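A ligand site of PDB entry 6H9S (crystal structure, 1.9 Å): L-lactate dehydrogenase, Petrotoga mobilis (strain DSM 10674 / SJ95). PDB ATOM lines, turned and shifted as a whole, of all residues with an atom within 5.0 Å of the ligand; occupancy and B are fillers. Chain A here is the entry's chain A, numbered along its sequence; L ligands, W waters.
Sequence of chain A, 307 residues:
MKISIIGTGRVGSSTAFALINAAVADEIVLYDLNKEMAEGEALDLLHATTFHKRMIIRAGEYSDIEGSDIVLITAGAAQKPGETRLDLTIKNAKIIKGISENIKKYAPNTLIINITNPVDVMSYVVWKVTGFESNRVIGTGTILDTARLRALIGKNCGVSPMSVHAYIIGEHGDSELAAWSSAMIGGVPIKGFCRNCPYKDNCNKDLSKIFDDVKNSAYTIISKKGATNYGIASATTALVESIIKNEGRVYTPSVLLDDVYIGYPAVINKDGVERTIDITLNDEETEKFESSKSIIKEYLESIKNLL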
ATOM      1  N   ILE A   6     -16.624   8.434 -26.739  1.00  0.00           N
ATOM      2  CA  ILE A   6     -17.166   8.522 -25.384  1.00  0.00           C
ATOM      3  C   ILE A   6     -18.006   9.793 -25.307  1.00  0.00           C
ATOM      4  O   ILE A   6     -17.471  10.902 -25.276  1.00  0.00           O
ATOM      5  CB  ILE A   6     -16.069   8.522 -24.313  1.00  0.00           C
ATOM      6  CG1 ILE A   6     -15.014   7.451 -24.599  1.00  0.00           C
ATOM      7  CG2 ILE A   6     -16.702   8.352 -22.912  1.00  0.00           C
ATOM      8  CD1 ILE A   6     -15.552   6.050 -24.810  1.00  0.00           C
ATOM      9  N   GLY A   7     -19.318   9.617 -25.219  1.00  0.00           N
ATOM     10  CA  GLY A   7     -20.251  10.727 -25.169  1.00  0.00           C
ATOM     11  C   GLY A   7     -20.946  10.843 -26.502  1.00  0.00           C
ATOM     12  O   GLY A   7     -20.423  11.451 -27.432  1.00  0.00           O
ATOM     13  N   THR A   8     -22.113  10.233 -26.633  1.00  0.00           N
ATOM     14  CA  THR A   8     -22.783  10.193 -27.941  1.00  0.00           C
ATOM     15  C   THR A   8     -23.910  11.216 -27.997  1.00  0.00           C
ATOM     16  O   THR A   8     -25.078  10.902 -28.247  1.00  0.00           O
ATOM     17  CB  THR A   8     -23.294   8.786 -28.213  1.00  0.00           C
ATOM     18  OG1 THR A   8     -24.463   8.541 -27.427  1.00  0.00           O
ATOM     19  CG2 THR A   8     -22.214   7.763 -27.848  1.00  0.00           C
ATOM     20  N   GLY A   9     -23.561  12.469 -27.727  1.00  0.00           N
ATOM     21  CA  GLY A   9     -24.485  13.593 -27.857  1.00  0.00           C
ATOM     22  C   GLY A   9     -24.445  14.176 -29.249  1.00  0.00           C
ATOM     23  O   GLY A   9     -24.221  13.483 -30.236  1.00  0.00           O
ATOM     24  N   ARG A  10     -24.653  15.497 -29.325  1.00  0.00           N
ATOM     25  CA  ARG A  10     -24.677  16.157 -30.631  1.00  0.00           C
ATOM     26  C   ARG A  10     -23.334  16.032 -31.328  1.00  0.00           C
ATOM     27  O   ARG A  10     -23.256  15.693 -32.513  1.00  0.00           O
ATOM     28  CB  ARG A  10     -25.089  17.633 -30.475  1.00  0.00           C
ATOM     29  CG  ARG A  10     -26.551  17.832 -30.045  1.00  0.00           C
ATOM     30  CD  ARG A  10     -26.829  19.247 -29.566  1.00  0.00           C
ATOM     31  NE  ARG A  10     -25.889  19.645 -28.515  1.00  0.00           N
ATOM     32  CZ  ARG A  10     -26.186  20.436 -27.493  1.00  0.00           C
ATOM     33  NH1 ARG A  10     -25.237  20.731 -26.602  1.00  0.00           N
ATOM     34  NH2 ARG A  10     -27.412  20.937 -27.342  1.00  0.00           N
ATOM     35  N   VAL A  11     -22.237  16.308 -30.605  1.00  0.00           N
ATOM     36  CA  VAL A  11     -20.914  16.254 -31.223  1.00  0.00           C
ATOM     37  C   VAL A  11     -20.518  14.805 -31.507  1.00  0.00           C
ATOM     38  O   VAL A  11     -19.986  14.480 -32.581  1.00  0.00           O
ATOM     39  CB  VAL A  11     -19.875  16.963 -30.333  1.00  0.00           C
ATOM     40  CG1 VAL A  11     -18.452  16.638 -30.827  1.00  0.00           C
ATOM     41  CG2 VAL A  11     -20.112  18.455 -30.345  1.00  0.00           C
ATOM     42  N   GLY A  12     -20.737  13.920 -30.531  1.00  0.00           N
ATOM     43  CA  GLY A  12     -20.319  12.533 -30.724  1.00  0.00           C
ATOM     44  C   GLY A  12     -21.022  11.879 -31.895  1.00  0.00           C
ATOM     45  O   GLY A  12     -20.391  11.210 -32.724  1.00  0.00           O
ATOM     46  N   TYR A  31     -20.213   5.031 -26.606  1.00  0.00           N
ATOM     47  CA  TYR A  31     -20.469   4.952 -25.168  1.00  0.00           C
ATOM     48  C   TYR A  31     -21.218   6.208 -24.716  1.00  0.00           C
ATOM     49  O   TYR A  31     -20.923   7.305 -25.182  1.00  0.00           O
ATOM     50  CB  TYR A  31     -19.162   4.835 -24.341  1.00  0.00           C
ATOM     51  CG  TYR A  31     -19.420   4.723 -22.854  1.00  0.00           C
ATOM     52  CD1 TYR A  31     -19.657   5.860 -22.079  1.00  0.00           C
ATOM     53  CD2 TYR A  31     -19.445   3.486 -22.211  1.00  0.00           C
ATOM     54  CE1 TYR A  31     -19.911   5.765 -20.712  1.00  0.00           C
ATOM     55  CE2 TYR A  31     -19.703   3.382 -20.834  1.00  0.00           C
ATOM     56  CZ  TYR A  31     -19.940   4.528 -20.099  1.00  0.00           C
ATOM     57  OH  TYR A  31     -20.189   4.420 -18.751  1.00  0.00           O
ATOM     58  N   ASP A  32     -22.168   6.023 -23.788  1.00  0.00           N
ATOM     59  CA  ASP A  32     -22.816   7.171 -23.163  1.00  0.00           C
ATOM     60  C   ASP A  32     -23.386   6.764 -21.811  1.00  0.00           C
ATOM     61  O   ASP A  32     -23.707   5.585 -21.590  1.00  0.00           O
ATOM     62  CB  ASP A  32     -23.906   7.782 -24.066  1.00  0.00           C
ATOM     63  CG  ASP A  32     -24.218   9.219 -23.689  1.00  0.00           C
ATOM     64  OD1 ASP A  32     -24.990   9.450 -22.745  1.00  0.00           O
ATOM     65  OD2 ASP A  32     -23.662  10.132 -24.329  1.00  0.00           O
ATOM     66  N   LEU A  33     -23.488   7.745 -20.909  1.00  0.00           N
ATOM     67  CA  LEU A  33     -24.222   7.544 -19.654  1.00  0.00           C
ATOM     68  C   LEU A  33     -25.669   7.143 -19.927  1.00  0.00           C
ATOM     69  O   LEU A  33     -26.257   6.362 -19.180  1.00  0.00           O
ATOM     70  CB  LEU A  33     -24.218   8.824 -18.814  1.00  0.00           C
ATOM     71  CG  LEU A  33     -22.985   9.259 -18.046  1.00  0.00           C
ATOM     72  CD1 LEU A  33     -23.377  10.407 -17.122  1.00  0.00           C
ATOM     73  CD2 LEU A  33     -22.379   8.111 -17.273  1.00  0.00           C
ATOM     74  N   ASN A  34     -26.269   7.732 -20.957  1.00  0.00           N
ATOM     75  CA  ASN A  34     -27.644   7.410 -21.348  1.00  0.00           C
ATOM     76  C   ASN A  34     -27.556   6.213 -22.284  1.00  0.00           C
ATOM     77  O   ASN A  34     -27.271   6.360 -23.477  1.00  0.00           O
ATOM     78  CB  ASN A  34     -28.302   8.620 -21.994  1.00  0.00           C
ATOM     79  CG  ASN A  34     -29.763   8.404 -22.282  1.00  0.00           C
ATOM     80  OD1 ASN A  34     -30.209   7.274 -22.507  1.00  0.00           O
ATOM     81  ND2 ASN A  34     -30.537   9.483 -22.272  1.00  0.00           N
ATOM     82  N   TYR A  62     -17.536   0.208 -21.255  1.00  0.00           N
ATOM     83  CA  TYR A  62     -16.120   0.529 -21.391  1.00  0.00           C
ATOM     84  C   TYR A  62     -15.305  -0.671 -21.846  1.00  0.00           C
ATOM     85  O   TYR A  62     -14.351  -0.533 -22.608  1.00  0.00           O
ATOM     86  CB  TYR A  62     -15.572   1.109 -20.085  1.00  0.00           C
ATOM     87  CG  TYR A  62     -15.782   2.605 -19.975  1.00  0.00           C
ATOM     88  CD1 TYR A  62     -15.227   3.472 -20.906  1.00  0.00           C
ATOM     89  CD2 TYR A  62     -16.532   3.151 -18.940  1.00  0.00           C
ATOM     90  CE1 TYR A  62     -15.420   4.843 -20.817  1.00  0.00           C
ATOM     91  CE2 TYR A  62     -16.728   4.521 -18.834  1.00  0.00           C
ATOM     92  CZ  TYR A  62     -16.165   5.362 -19.784  1.00  0.00           C
ATOM     93  OH  TYR A  62     -16.359   6.726 -19.702  1.00  0.00           O
ATOM     94  N   THR A  74     -16.042  13.071 -26.369  1.00  0.00           N
ATOM     95  CA  THR A  74     -17.000  14.084 -26.771  1.00  0.00           C
ATOM     96  C   THR A  74     -18.126  14.199 -25.740  1.00  0.00           C
ATOM     97  O   THR A  74     -19.250  14.563 -26.079  1.00  0.00           O
ATOM     98  CB  THR A  74     -17.548  13.776 -28.157  1.00  0.00           C
ATOM     99  OG1 THR A  74     -18.040  12.430 -28.187  1.00  0.00           O
ATOM    100  CG2 THR A  74     -16.432  13.900 -29.214  1.00  0.00           C
ATOM    101  N   ALA A  75     -17.814  13.922 -24.487  1.00  0.00           N
ATOM    102  CA  ALA A  75     -18.763  13.979 -23.385  1.00  0.00           C
ATOM    103  C   ALA A  75     -18.790  15.376 -22.779  1.00  0.00           C
ATOM    104  O   ALA A  75     -17.955  16.240 -23.074  1.00  0.00           O
ATOM    105  CB  ALA A  75     -18.397  12.967 -22.304  1.00  0.00           C
ATOM    106  N   GLY A  76     -19.768  15.601 -21.904  1.00  0.00           N
ATOM    107  CA  GLY A  76     -19.780  16.898 -21.271  1.00  0.00           C
ATOM    108  C   GLY A  76     -21.056  17.199 -20.542  1.00  0.00           C
ATOM    109  O   GLY A  76     -22.092  16.595 -20.818  1.00  0.00           O
ATOM    110  N   ALA A  77     -20.976  18.132 -19.596  1.00  0.00           N
ATOM    111  CA  ALA A  77     -22.136  18.479 -18.800  1.00  0.00           C
ATOM    112  C   ALA A  77     -23.129  19.269 -19.637  1.00  0.00           C
ATOM    113  O   ALA A  77     -22.792  19.885 -20.657  1.00  0.00           O
ATOM    114  CB  ALA A  77     -21.694  19.283 -17.581  1.00  0.00           C
ATOM    115  N   ASN A  92     -16.796  19.507 -15.960  1.00  0.00           N
ATOM    116  CA  ASN A  92     -16.245  18.626 -16.972  1.00  0.00           C
ATOM    117  C   ASN A  92     -14.963  17.937 -16.513  1.00  0.00           C
ATOM    118  O   ASN A  92     -14.670  16.819 -16.968  1.00  0.00           O
ATOM    119  CB  ASN A  92     -16.013  19.391 -18.268  1.00  0.00           C
ATOM    120  CG  ASN A  92     -17.305  19.650 -19.026  1.00  0.00           C
ATOM    121  OD1 ASN A  92     -18.359  19.122 -18.654  1.00  0.00           O
ATOM    122  ND2 ASN A  92     -17.232  20.441 -20.084  1.00  0.00           N
ATOM    123  N   ILE A  95     -15.962  14.735 -15.029  1.00  0.00           N
ATOM    124  CA  ILE A  95     -16.363  13.820 -16.082  1.00  0.00           C
ATOM    125  C   ILE A  95     -15.128  13.235 -16.767  1.00  0.00           C
ATOM    126  O   ILE A  95     -15.026  12.019 -16.965  1.00  0.00           O
ATOM    127  CB  ILE A  95     -17.278  14.549 -17.084  1.00  0.00           C
ATOM    128  CG1 ILE A  95     -18.646  14.839 -16.451  1.00  0.00           C
ATOM    129  CG2 ILE A  95     -17.392  13.750 -18.398  1.00  0.00           C
ATOM    130  CD1 ILE A  95     -19.517  15.815 -17.237  1.00  0.00           C
ATOM    131  N   ILE A  99     -13.715   9.269 -17.196  1.00  0.00           N
ATOM    132  CA  ILE A  99     -13.495   8.699 -18.518  1.00  0.00           C
ATOM    133  C   ILE A  99     -12.043   8.279 -18.683  1.00  0.00           C
ATOM    134  O   ILE A  99     -11.748   7.202 -19.228  1.00  0.00           O
ATOM    135  CB  ILE A  99     -13.913   9.709 -19.612  1.00  0.00           C
ATOM    136  CG1 ILE A  99     -15.431   9.909 -19.582  1.00  0.00           C
ATOM    137  CG2 ILE A  99     -13.410   9.260 -20.977  1.00  0.00           C
ATOM    138  CD1 ILE A  99     -15.900  11.108 -20.402  1.00  0.00           C
ATOM    139  N   ILE A 115     -12.235  16.444 -27.166  1.00  0.00           N
ATOM    140  CA  ILE A 115     -13.024  17.549 -27.711  1.00  0.00           C
ATOM    141  C   ILE A 115     -13.700  18.311 -26.569  1.00  0.00           C
ATOM    142  O   ILE A 115     -13.997  19.497 -26.700  1.00  0.00           O
ATOM    143  CB  ILE A 115     -14.075  17.063 -28.728  1.00  0.00           C
ATOM    144  CG1 ILE A 115     -13.426  16.580 -30.023  1.00  0.00           C
ATOM    145  CG2 ILE A 115     -15.110  18.149 -29.022  1.00  0.00           C
ATOM    146  CD1 ILE A 115     -13.012  15.127 -29.983  1.00  0.00           C
ATOM    147  N   THR A 116     -13.952  17.627 -25.456  1.00  0.00           N
ATOM    148  CA  THR A 116     -14.659  18.233 -24.334  1.00  0.00           C
ATOM    149  C   THR A 116     -13.997  19.542 -23.898  1.00  0.00           C
ATOM    150  O   THR A 116     -12.769  19.623 -23.790  1.00  0.00           O
ATOM    151  CB  THR A 116     -14.684  17.255 -23.152  1.00  0.00           C
ATOM    152  OG1 THR A 116     -15.308  16.039 -23.562  1.00  0.00           O
ATOM    153  CG2 THR A 116     -15.478  17.855 -21.954  1.00  0.00           C
ATOM    154  N   ASN A 117     -14.826  20.570 -23.613  1.00  0.00           N
ATOM    155  CA  ASN A 117     -14.353  21.913 -23.265  1.00  0.00           C
ATOM    156  C   ASN A 117     -14.162  22.088 -21.758  1.00  0.00           C
ATOM    157  O   ASN A 117     -14.829  21.417 -20.959  1.00  0.00           O
ATOM    158  CB  ASN A 117     -15.336  22.963 -23.743  1.00  0.00           C
ATOM    159  CG  ASN A 117     -15.080  23.380 -25.167  1.00  0.00           C
ATOM    160  OD1 ASN A 117     -13.936  23.446 -25.611  1.00  0.00           O
ATOM    161  ND2 ASN A 117     -16.157  23.657 -25.900  1.00  0.00           N
ATOM    162  N   VAL A 119     -11.110  22.817 -24.117  1.00  0.00           N
ATOM    163  CA  VAL A 119     -10.430  21.690 -24.760  1.00  0.00           C
ATOM    164  C   VAL A 119      -8.970  21.577 -24.304  1.00  0.00           C
ATOM    165  O   VAL A 119      -8.451  20.474 -24.129  1.00  0.00           O
ATOM    166  CB  VAL A 119     -10.562  21.796 -26.296  1.00  0.00           C
ATOM    167  CG1 VAL A 119      -9.804  23.000 -26.840  1.00  0.00           C
ATOM    168  CG2 VAL A 119     -10.084  20.503 -26.958  1.00  0.00           C
ATOM    169  N   THR A 140      -8.478  18.922 -29.844  1.00  0.00           N
ATOM    170  CA  THR A 140      -8.696  19.502 -31.161  1.00  0.00           C
ATOM    171  C   THR A 140      -8.252  20.955 -31.245  1.00  0.00           C
ATOM    172  O   THR A 140      -8.232  21.501 -32.356  1.00  0.00           O
ATOM    173  CB  THR A 140     -10.156  19.381 -31.562  1.00  0.00           C
ATOM    174  OG1 THR A 140     -10.986  19.881 -30.501  1.00  0.00           O
ATOM    175  CG2 THR A 140     -10.501  17.912 -31.828  1.00  0.00           C
ATOM    176  N   GLY A 141      -7.936  21.590 -30.124  1.00  0.00           N
ATOM    177  CA  GLY A 141      -7.269  22.880 -30.157  1.00  0.00           C
ATOM    178  C   GLY A 141      -7.926  23.906 -31.084  1.00  0.00           C
ATOM    179  O   GLY A 141      -9.135  24.149 -31.036  1.00  0.00           O
ATOM    180  N   HIS A 172      -7.901  27.895 -27.221  1.00  0.00           N
ATOM    181  CA  HIS A 172      -9.061  27.899 -28.102  1.00  0.00           C
ATOM    182  C   HIS A 172     -10.160  28.785 -27.535  1.00  0.00           C
ATOM    183  O   HIS A 172     -10.600  28.590 -26.397  1.00  0.00           O
ATOM    184  CB  HIS A 172      -9.587  26.471 -28.302  1.00  0.00           C
ATOM    185  CG  HIS A 172     -10.825  26.400 -29.142  1.00  0.00           C
ATOM    186  ND1 HIS A 172     -11.998  25.815 -28.692  1.00  0.00           N
ATOM    187  CD2 HIS A 172     -11.092  26.843 -30.391  1.00  0.00           C
ATOM    188  CE1 HIS A 172     -12.922  25.890 -29.639  1.00  0.00           C
ATOM    189  NE2 HIS A 172     -12.389  26.515 -30.678  1.00  0.00           N
ATOM    190  N   ALA A 227     -25.996  25.216 -29.733  1.00  0.00           N
ATOM    191  CA  ALA A 227     -24.718  24.521 -29.620  1.00  0.00           C
ATOM    192  C   ALA A 227     -24.064  24.505 -30.994  1.00  0.00           C
ATOM    193  O   ALA A 227     -24.629  24.976 -31.983  1.00  0.00           O
ATOM    194  CB  ALA A 227     -24.913  23.126 -29.045  1.00  0.00           C
ATOM    195  N   THR A 228     -22.850  23.961 -31.052  1.00  0.00           N
ATOM    196  CA  THR A 228     -22.124  23.785 -32.307  1.00  0.00           C
ATOM    197  C   THR A 228     -21.638  22.347 -32.391  1.00  0.00           C
ATOM    198  O   THR A 228     -21.280  21.755 -31.366  1.00  0.00           O
ATOM    199  CB  THR A 228     -20.943  24.775 -32.432  1.00  0.00           C
ATOM    200  OG1 THR A 228     -20.374  24.674 -33.738  1.00  0.00           O
ATOM    201  CG2 THR A 228     -19.866  24.485 -31.390  1.00  0.00           C
ATOM    202  N   ILE A 232     -16.857  21.066 -35.697  1.00  0.00           N
ATOM    203  CA  ILE A 232     -15.879  20.265 -34.962  1.00  0.00           C
ATOM    204  C   ILE A 232     -15.905  18.805 -35.429  1.00  0.00           C
ATOM    205  O   ILE A 232     -14.853  18.149 -35.472  1.00  0.00           O
ATOM    206  CB  ILE A 232     -16.125  20.384 -33.440  1.00  0.00           C
ATOM    207  CG1 ILE A 232     -15.048  19.620 -32.653  1.00  0.00           C
ATOM    208  CG2 ILE A 232     -17.502  19.865 -33.047  1.00  0.00           C
ATOM    209  CD1 ILE A 232     -13.623  20.118 -32.918  1.00  0.00           C
HETATM  210  P1  LIG L   1     -24.305  17.031 -25.569  1.00  0.00           P
HETATM  211  O1  LIG L   1     -25.039  17.457 -24.309  1.00  0.00           O
HETATM  212  O2  LIG L   1     -25.215  17.003 -26.781  1.00  0.00           O
HETATM  213  O3  LIG L   1     -23.627  15.548 -25.408  1.00  0.00           O
HETATM  214  C1  LIG L   1     -22.836  15.285 -24.286  1.00  0.00           C
HETATM  215  C2  LIG L   1     -22.921  13.762 -23.977  1.00  0.00           C
HETATM  216  O4  LIG L   1     -22.073  13.462 -23.009  1.00  0.00           O
HETATM  217  C3  LIG L   1     -24.342  13.386 -23.472  1.00  0.00           C
HETATM  218  O5  LIG L   1     -24.872  12.417 -24.285  1.00  0.00           O
HETATM  219  C4  LIG L   1     -24.083  12.899 -22.012  1.00  0.00           C
HETATM  220  O6  LIG L   1     -25.045  11.821 -21.677  1.00  0.00           O
HETATM  221  C5  LIG L   1     -22.861  12.414 -22.074  1.00  0.00           C
HETATM  222  N1  LIG L   1     -22.172  12.346 -20.820  1.00  0.00           N
HETATM  223  C6  LIG L   1     -22.309  13.204 -19.793  1.00  0.00           C
HETATM  224  N2  LIG L   1     -21.528  12.789 -18.804  1.00  0.00           N
HETATM  225  C7  LIG L   1     -20.885  11.685 -19.239  1.00  0.00           C
HETATM  226  C8  LIG L   1     -19.984  10.870 -18.615  1.00  0.00           C
HETATM  227  N3  LIG L   1     -19.360  10.865 -17.306  1.00  0.00           N
HETATM  228  N4  LIG L   1     -19.485   9.809 -19.247  1.00  0.00           N
HETATM  229  C9  LIG L   1     -19.906   9.532 -20.508  1.00  0.00           C
HETATM  230  N5  LIG L   1     -20.803  10.340 -21.126  1.00  0.00           N
HETATM  231  C10 LIG L   1     -21.293  11.408 -20.474  1.00  0.00           C
HETATM  232  O7  LIG L   1     -23.100  18.109 -25.764  1.00  0.00           O
HETATM  233  P2  LIG L   1     -22.290  18.328 -27.177  1.00  0.00           P
HETATM  234  O8  LIG L   1     -22.942  19.426 -27.973  1.00  0.00           O
HETATM  235  O9  LIG L   1     -22.260  17.006 -27.921  1.00  0.00           O
HETATM  236  O10 LIG L   1     -20.817  18.806 -26.682  1.00  0.00           O
HETATM  237  C11 LIG L   1     -20.044  17.834 -26.020  1.00  0.00           C
HETATM  238  C12 LIG L   1     -18.702  18.493 -25.591  1.00  0.00           C
HETATM  239  O11 LIG L   1     -18.027  18.901 -26.648  1.00  0.00           O
HETATM  240  C13 LIG L   1     -18.976  19.756 -24.746  1.00  0.00           C
HETATM  241  O12 LIG L   1     -18.072  19.838 -23.722  1.00  0.00           O
HETATM  242  C14 LIG L   1     -18.737  20.920 -25.740  1.00  0.00           C
HETATM  243  O13 LIG L   1     -18.378  22.166 -25.007  1.00  0.00           O
HETATM  244  C15 LIG L   1     -17.703  20.460 -26.382  1.00  0.00           C
HETATM  245  N6  LIG L   1     -17.419  21.038 -27.659  1.00  0.00           N
HETATM  246  C16 LIG L   1     -16.117  21.276 -27.942  1.00  0.00           C
HETATM  247  C17 LIG L   1     -15.758  21.856 -29.137  1.00  0.00           C
HETATM  248  C18 LIG L   1     -14.277  22.096 -29.383  1.00  0.00           C
HETATM  249  O14 LIG L   1     -13.454  21.531 -28.736  1.00  0.00           O
HETATM  250  N7  LIG L   1     -13.883  23.010 -30.409  1.00  0.00           N
HETATM  251  C19 LIG L   1     -16.707  22.183 -30.047  1.00  0.00           C
HETATM  252  C20 LIG L   1     -18.018  21.944 -29.759  1.00  0.00           C
HETATM  253  C21 LIG L   1     -18.373  21.357 -28.558  1.00  0.00           C
HETATM  254  O   HOH W   1     -11.236  22.482 -30.523  1.00  0.00           O
HETATM  255  O   HOH W   2     -27.517  15.496 -26.749  1.00  0.00           O
HETATM  256  O   HOH W   3     -20.599  12.188 -14.914  1.00  0.00           O
HETATM  257  O   HOH W   4     -19.832  20.949 -21.704  1.00  0.00           O
HETATM  258  O   HOH W   5     -18.223   7.591 -17.973  1.00  0.00           O
HETATM  259  O   HOH W   6     -22.555  13.774 -16.368  1.00  0.00           O
HETATM  260  O   HOH W   7     -27.638  13.337 -25.421  1.00  0.00           O
HETATM  261  O   HOH W   8     -21.710  21.562 -28.815  1.00  0.00           O
HETATM  262  O   HOH W   9     -21.468  14.477 -27.771  1.00  0.00           O
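The backbone carbonyl oxygen of Ile 115 sits close to an oxygen (O14) of the ligand (2.9 Å).
Merely in contact with the ligand: Gly 7 (3.9 Å), Gly 9 (3.2 Å), Tyr 31 (3.8 Å), Leu 33 (3.4 Å), Thr 74 (3.4 Å), Ala 75 (3.4 Å), Asn 92 (3.8 Å), Ile 95 (3.7 Å), Ile 99 (3.98 Å), Thr 116 (3.7 Å), Val 119 (3.8 Å), His 172 (3.1 Å), Thr 228 (3.5 Å) and Ile 232 (3.8 Å).
Hydrophobic or aromatic side chains that line the ligand: Val 11, Tyr 31, Leu 33, Ala 75, Ile 95, Ile 99, Ile 115, Val 119, His 172 and Ile 232.
Within 4 Å of the ligand: Gly 7, Gly 9, Arg 10, Val 11, Tyr 31, Asp 32, Leu 33, Thr 74, Ala 75, Gly 76, Asn 92, Ile 95, Ile 99, Ile 115, Thr 116, Asn 117, Val 119, Thr 140, His 172, Thr 228 and Ile 232.
Water W8 bridges O of Thr 228 and O8 of the ligand.
Water W1 lies within hydrogen-bond range of OG1 of Thr 140 (2.6 Å), N7 of the ligand (2.7 Å) and O of Gly 141 (2.7 Å).
Water W5 lies within hydrogen-bond range of the side-chain hydroxyl of Tyr 62 (2.7 Å) and a nitrogen (N4) of the ligand (2.9 Å).
Water W4 lies within hydrogen-bond range of an oxygen (O12) of the ligand (2.9 Å), the side-chain amide nitrogen (ND2) of Asn 92 (3.1 Å) and the backbone carbonyl oxygen (O) of Ala 77 (3.3 Å).
The side-chain carboxylate (OD2) of Asp 32 lies within hydrogen-bond range of an oxygen (O5) of the ligand, 2.6 Å away.
The backbone NH (N) of Val 11 sits at hydrogen-bond distance from an oxygen (O9) of the ligand (2.8 Å).
O12 of the ligand is in hydrogen-bond range of N of Asn 117 (3.3 Å).
An oxygen (O13) of the ligand is in hydrogen-bond range of the side-chain amide nitrogen of Asn 117 (2.8 Å).
The backbone NH of Arg 10 is in hydrogen-bond range of an oxygen (O2) of the ligand (3.0 Å).
An oxygen (O8) of the ligand lies within salt-bridge range of the guanidinium group (NH1) of Arg 10.
An oxygen (O4) of the ligand sits at hydrogen-bond distance from the backbone NH (N) of Gly 76 (3.3 Å).
An oxygen (O14) of the ligand lies within hydrogen-bond range of the side-chain hydroxyl (OG1) of Thr 140 (3.5 Å).
The side-chain carboxylate of Asp 32 lies within hydrogen-bond range of the backbone NH of Thr 8 (2.8 Å).
The backbone NH (N) of Val 119 is in hydrogen-bond range of the side-chain amide oxygen (OD1) of Asn 117 (3.3 Å).
O of Gly 7 sits at hydrogen-bond distance from OG1 of Thr 74, at 2.7 Å.
The backbone NH of Thr 74 lies within hydrogen-bond range of the backbone carbonyl oxygen of Ile 6, 2.8 Å away.
The side-chain hydroxyl (OG1) of Thr 116 is in hydrogen-bond range of the backbone carbonyl oxygen (O) of Ala 75, at 2.7 Å.
The backbone carbonyl oxygen of Ile 6 sits at hydrogen-bond distance from the backbone NH of Ala 75 (3.1 Å).
N of Gly 7 sits at hydrogen-bond distance from O of Tyr 31.
The side-chain amide oxygen (OD1) of Asn 92 lies within hydrogen-bond range of the backbone NH (N) of Ala 77.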
